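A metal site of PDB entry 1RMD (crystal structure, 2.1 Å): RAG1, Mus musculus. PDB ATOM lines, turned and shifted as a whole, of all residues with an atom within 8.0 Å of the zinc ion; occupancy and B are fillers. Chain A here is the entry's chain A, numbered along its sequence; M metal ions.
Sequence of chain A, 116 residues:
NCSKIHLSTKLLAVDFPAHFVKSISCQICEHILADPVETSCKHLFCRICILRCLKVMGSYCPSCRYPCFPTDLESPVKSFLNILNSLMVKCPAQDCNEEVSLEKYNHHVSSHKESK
Residues that only touch the zinc ion: Ala 93.
Five residues have an atom within 4 Å of the zinc ion: Cys 91, Ala 93, Cys 96, His 108 and His 112.
The nearest printed residue that does not touch the zinc ion is Glu 98 (4.7 Å).
The zinc ion is bound by NE2 of His 112 (2.0 Å), NE2 of His 108 (2.0 Å), SG of Cys 91 (2.3 Å) and SG of Cys 96 (2.4 Å).
The zinc ion has four donor atoms within binding distance.
O of His 108 is in hydrogen-bond range of OG of Ser 111, at 2.9 Å.
The side-chain sulfur (SG) of Cys 91 sits close to the backbone NH (N) of Ala 93 (3.5 Å).
The backbone NH (N) of Cys 91 sits at hydrogen-bond distance from the backbone carbonyl oxygen (O) of Glu 98.
N of Glu 98 sits close to SG of Cys 96 (3.7 Å).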
ATOM      1  N   VAL A  89      13.422 -27.045  12.560  1.00  0.00           N
ATOM      2  CA  VAL A  89      12.870 -28.117  11.739  1.00  0.00           C
ATOM      3  C   VAL A  89      12.657 -27.702  10.276  1.00  0.00           C
ATOM      4  O   VAL A  89      12.316 -26.561   9.984  1.00  0.00           O
ATOM      5  CB  VAL A  89      11.580 -28.680  12.398  1.00  0.00           C
ATOM      6  CG1 VAL A  89      10.920 -27.605  13.251  1.00  0.00           C
ATOM      7  CG2 VAL A  89      10.622 -29.235  11.343  1.00  0.00           C
ATOM      8  N   LYS A  90      12.991 -28.623   9.369  1.00  0.00           N
ATOM      9  CA  LYS A  90      12.841 -28.406   7.949  1.00  0.00           C
ATOM     10  C   LYS A  90      11.416 -28.694   7.484  1.00  0.00           C
ATOM     11  O   LYS A  90      10.975 -29.844   7.442  1.00  0.00           O
ATOM     12  CB  LYS A  90      13.815 -29.300   7.151  1.00  0.00           C
ATOM     13  CG  LYS A  90      15.289 -28.888   7.245  1.00  0.00           C
ATOM     14  CD  LYS A  90      16.218 -29.963   6.668  1.00  0.00           C
ATOM     15  CE  LYS A  90      15.975 -31.301   7.365  1.00  0.00           C
ATOM     16  NZ  LYS A  90      16.838 -32.393   6.863  1.00  0.00           N
ATOM     17  N   CYS A  91      10.717 -27.629   7.104  1.00  0.00           N
ATOM     18  CA  CYS A  91       9.340 -27.735   6.604  1.00  0.00           C
ATOM     19  C   CYS A  91       9.393 -28.573   5.332  1.00  0.00           C
ATOM     20  O   CYS A  91      10.208 -28.335   4.459  1.00  0.00           O
ATOM     21  CB  CYS A  91       8.784 -26.339   6.320  1.00  0.00           C
ATOM     22  SG  CYS A  91       7.250 -26.344   5.399  1.00  0.00           S
ATOM     23  N   PRO A  92       8.564 -29.631   5.246  1.00  0.00           N
ATOM     24  CA  PRO A  92       8.482 -30.558   4.107  1.00  0.00           C
ATOM     25  C   PRO A  92       7.480 -30.162   2.994  1.00  0.00           C
ATOM     26  O   PRO A  92       7.237 -30.910   2.044  1.00  0.00           O
ATOM     27  CB  PRO A  92       8.092 -31.872   4.780  1.00  0.00           C
ATOM     28  CG  PRO A  92       7.116 -31.411   5.843  1.00  0.00           C
ATOM     29  CD  PRO A  92       7.712 -30.083   6.372  1.00  0.00           C
ATOM     30  N   ALA A  93       6.887 -28.989   3.129  1.00  0.00           N
ATOM     31  CA  ALA A  93       5.962 -28.536   2.110  1.00  0.00           C
ATOM     32  C   ALA A  93       6.751 -28.399   0.796  1.00  0.00           C
ATOM     33  O   ALA A  93       7.846 -27.840   0.793  1.00  0.00           O
ATOM     34  CB  ALA A  93       5.367 -27.186   2.506  1.00  0.00           C
ATOM     35  N   GLN A  94       6.189 -28.923  -0.295  1.00  0.00           N
ATOM     36  CA  GLN A  94       6.807 -28.896  -1.623  1.00  0.00           C
ATOM     37  C   GLN A  94       7.465 -27.568  -2.032  1.00  0.00           C
ATOM     38  O   GLN A  94       6.809 -26.524  -1.990  1.00  0.00           O
ATOM     39  CB  GLN A  94       5.753 -29.287  -2.649  1.00  0.00           C
ATOM     40  CG  GLN A  94       6.210 -29.422  -4.080  1.00  0.00           C
ATOM     41  CD  GLN A  94       5.104 -29.987  -4.970  1.00  0.00           C
ATOM     42  OE1 GLN A  94       3.937 -29.618  -4.857  1.00  0.00           O
ATOM     43  NE2 GLN A  94       5.478 -30.914  -5.851  1.00  0.00           N
ATOM     44  N   ASP A  95       8.745 -27.610  -2.397  1.00  0.00           N
ATOM     45  CA  ASP A  95       9.511 -26.431  -2.819  1.00  0.00           C
ATOM     46  C   ASP A  95       9.841 -25.379  -1.767  1.00  0.00           C
ATOM     47  O   ASP A  95      10.509 -24.383  -2.055  1.00  0.00           O
ATOM     48  CB  ASP A  95       8.871 -25.748  -4.016  1.00  0.00           C
ATOM     49  CG  ASP A  95       9.290 -26.380  -5.324  1.00  0.00           C
ATOM     50  OD1 ASP A  95      10.384 -26.026  -5.825  1.00  0.00           O
ATOM     51  OD2 ASP A  95       8.535 -27.241  -5.831  1.00  0.00           O
ATOM     52  N   CYS A  96       9.330 -25.575  -0.550  1.00  0.00           N
ATOM     53  CA  CYS A  96       9.629 -24.663   0.539  1.00  0.00           C
ATOM     54  C   CYS A  96      10.948 -25.148   1.123  1.00  0.00           C
ATOM     55  O   CYS A  96      11.114 -26.331   1.463  1.00  0.00           O
ATOM     56  CB  CYS A  96       8.538 -24.709   1.606  1.00  0.00           C
ATOM     57  SG  CYS A  96       8.945 -23.687   3.010  1.00  0.00           S
ATOM     58  N   ASN A  97      11.917 -24.247   1.204  1.00  0.00           N
ATOM     59  CA  ASN A  97      13.203 -24.641   1.741  1.00  0.00           C
ATOM     60  C   ASN A  97      13.465 -23.783   2.949  1.00  0.00           C
ATOM     61  O   ASN A  97      14.517 -23.128   3.088  1.00  0.00           O
ATOM     62  CB  ASN A  97      14.298 -24.505   0.676  1.00  0.00           C
ATOM     63  CG  ASN A  97      14.077 -25.459  -0.499  1.00  0.00           C
ATOM     64  OD1 ASN A  97      14.445 -26.636  -0.446  1.00  0.00           O
ATOM     65  ND2 ASN A  97      13.438 -24.958  -1.561  1.00  0.00           N
ATOM     66  N   GLU A  98      12.498 -23.818   3.851  1.00  0.00           N
ATOM     67  CA  GLU A  98      12.543 -23.025   5.050  1.00  0.00           C
ATOM     68  C   GLU A  98      12.670 -23.884   6.290  1.00  0.00           C
ATOM     69  O   GLU A  98      12.118 -24.980   6.381  1.00  0.00           O
ATOM     70  CB  GLU A  98      11.300 -22.144   5.123  1.00  0.00           C
ATOM     71  CG  GLU A  98      11.532 -20.682   4.815  1.00  0.00           C
ATOM     72  CD  GLU A  98      11.369 -19.824   6.057  1.00  0.00           C
ATOM     73  OE1 GLU A  98      12.279 -19.855   6.918  1.00  0.00           O
ATOM     74  OE2 GLU A  98      10.322 -19.161   6.204  1.00  0.00           O
ATOM     75  N   GLU A  99      13.450 -23.375   7.231  1.00  0.00           N
ATOM     76  CA  GLU A  99      13.669 -24.039   8.492  1.00  0.00           C
ATOM     77  C   GLU A  99      13.139 -23.085   9.560  1.00  0.00           C
ATOM     78  O   GLU A  99      13.392 -21.886   9.495  1.00  0.00           O
ATOM     79  CB  GLU A  99      15.176 -24.298   8.669  1.00  0.00           C
ATOM     80  CG  GLU A  99      15.788 -25.032   7.471  1.00  0.00           C
ATOM     81  CD  GLU A  99      17.187 -25.627   7.722  1.00  0.00           C
ATOM     82  OE1 GLU A  99      17.837 -25.263   8.721  1.00  0.00           O
ATOM     83  OE2 GLU A  99      17.629 -26.463   6.903  1.00  0.00           O
ATOM     84  N   VAL A 100      12.350 -23.596  10.498  1.00  0.00           N
ATOM     85  CA  VAL A 100      11.800 -22.763  11.574  1.00  0.00           C
ATOM     86  C   VAL A 100      11.807 -23.512  12.914  1.00  0.00           C
ATOM     87  O   VAL A 100      11.856 -24.756  12.948  1.00  0.00           O
ATOM     88  CB  VAL A 100      10.329 -22.352  11.281  1.00  0.00           C
ATOM     89  CG1 VAL A 100      10.242 -21.455  10.063  1.00  0.00           C
ATOM     90  CG2 VAL A 100       9.460 -23.579  11.084  1.00  0.00           C
ATOM     91  N   TYR A 105       6.569 -23.257  14.223  1.00  0.00           N
ATOM     92  CA  TYR A 105       6.168 -24.141  13.155  1.00  0.00           C
ATOM     93  C   TYR A 105       4.708 -24.062  12.731  1.00  0.00           C
ATOM     94  O   TYR A 105       4.430 -23.826  11.574  1.00  0.00           O
ATOM     95  CB  TYR A 105       6.544 -25.567  13.466  1.00  0.00           C
ATOM     96  CG  TYR A 105       6.376 -26.498  12.299  1.00  0.00           C
ATOM     97  CD1 TYR A 105       7.341 -26.573  11.297  1.00  0.00           C
ATOM     98  CD2 TYR A 105       5.276 -27.349  12.229  1.00  0.00           C
ATOM     99  CE1 TYR A 105       7.210 -27.480  10.255  1.00  0.00           C
ATOM    100  CE2 TYR A 105       5.149 -28.255  11.196  1.00  0.00           C
ATOM    101  CZ  TYR A 105       6.101 -28.329  10.221  1.00  0.00           C
ATOM    102  OH  TYR A 105       5.933 -29.256   9.208  1.00  0.00           O
ATOM    103  N   HIS A 108       4.043 -21.121  10.739  1.00  0.00           N
ATOM    104  CA  HIS A 108       4.650 -21.188   9.412  1.00  0.00           C
ATOM    105  C   HIS A 108       3.799 -22.045   8.509  1.00  0.00           C
ATOM    106  O   HIS A 108       3.615 -21.697   7.335  1.00  0.00           O
ATOM    107  CB  HIS A 108       6.067 -21.782   9.447  1.00  0.00           C
ATOM    108  CG  HIS A 108       6.607 -22.130   8.085  1.00  0.00           C
ATOM    109  ND1 HIS A 108       7.086 -21.201   7.185  1.00  0.00           N
ATOM    110  CD2 HIS A 108       6.712 -23.322   7.455  1.00  0.00           C
ATOM    111  CE1 HIS A 108       7.455 -21.846   6.065  1.00  0.00           C
ATOM    112  NE2 HIS A 108       7.256 -23.145   6.159  1.00  0.00           N
ATOM    113  N   VAL A 109       3.319 -23.180   9.010  1.00  0.00           N
ATOM    114  CA  VAL A 109       2.504 -24.039   8.178  1.00  0.00           C
ATOM    115  C   VAL A 109       1.273 -23.295   7.698  1.00  0.00           C
ATOM    116  O   VAL A 109       1.065 -23.197   6.488  1.00  0.00           O
ATOM    117  CB  VAL A 109       2.135 -25.398   8.845  1.00  0.00           C
ATOM    118  CG1 VAL A 109       3.397 -26.200   9.097  1.00  0.00           C
ATOM    119  CG2 VAL A 109       1.389 -25.204  10.147  1.00  0.00           C
ATOM    120  N   SER A 110       0.553 -22.667   8.635  1.00  0.00           N
ATOM    121  CA  SER A 110      -0.671 -21.940   8.328  1.00  0.00           C
ATOM    122  C   SER A 110      -0.421 -20.808   7.349  1.00  0.00           C
ATOM    123  O   SER A 110      -1.066 -20.710   6.299  1.00  0.00           O
ATOM    124  CB  SER A 110      -1.289 -21.362   9.597  1.00  0.00           C
ATOM    125  OG  SER A 110      -0.618 -20.170   9.983  1.00  0.00           O
ATOM    126  N   SER A 111       0.564 -19.986   7.680  1.00  0.00           N
ATOM    127  CA  SER A 111       0.911 -18.857   6.822  1.00  0.00           C
ATOM    128  C   SER A 111       1.276 -19.266   5.389  1.00  0.00           C
ATOM    129  O   SER A 111       1.433 -18.412   4.527  1.00  0.00           O
ATOM    130  CB  SER A 111       2.041 -18.063   7.475  1.00  0.00           C
ATOM    131  OG  SER A 111       3.185 -18.879   7.671  1.00  0.00           O
ATOM    132  N   HIS A 112       1.425 -20.563   5.142  1.00  0.00           N
ATOM    133  CA  HIS A 112       1.770 -21.059   3.801  1.00  0.00           C
ATOM    134  C   HIS A 112       0.665 -20.597   2.850  1.00  0.00           C
ATOM    135  O   HIS A 112      -0.520 -20.738   3.166  1.00  0.00           O
ATOM    136  CB  HIS A 112       1.846 -22.594   3.781  1.00  0.00           C
ATOM    137  CG  HIS A 112       3.234 -23.131   3.616  1.00  0.00           C
ATOM    138  ND1 HIS A 112       3.874 -23.262   2.390  1.00  0.00           N
ATOM    139  CD2 HIS A 112       4.119 -23.602   4.534  1.00  0.00           C
ATOM    140  CE1 HIS A 112       5.093 -23.790   2.595  1.00  0.00           C
ATOM    141  NE2 HIS A 112       5.293 -24.012   3.884  1.00  0.00           N
ATOM    142  N   LYS A 113       1.054 -20.033   1.700  1.00  0.00           N
ATOM    143  CA  LYS A 113       0.080 -19.551   0.711  1.00  0.00           C
ATOM    144  C   LYS A 113      -0.541 -20.727  -0.060  1.00  0.00           C
ATOM    145  O   LYS A 113       0.169 -21.563  -0.603  1.00  0.00           O
ATOM    146  CB  LYS A 113       0.775 -18.571  -0.246  1.00  0.00           C
ATOM    147  CG  LYS A 113      -0.141 -17.701  -1.105  1.00  0.00           C
ATOM    148  CD  LYS A 113      -0.855 -16.627  -0.262  1.00  0.00           C
ATOM    149  CE  LYS A 113      -1.633 -15.634  -1.160  1.00  0.00           C
ATOM    150  NZ  LYS A 113      -2.509 -14.667  -0.411  1.00  0.00           N
HETATM  151 ZN    ZN M   1       7.141 -24.222   4.487  1.00  0.00          ZN
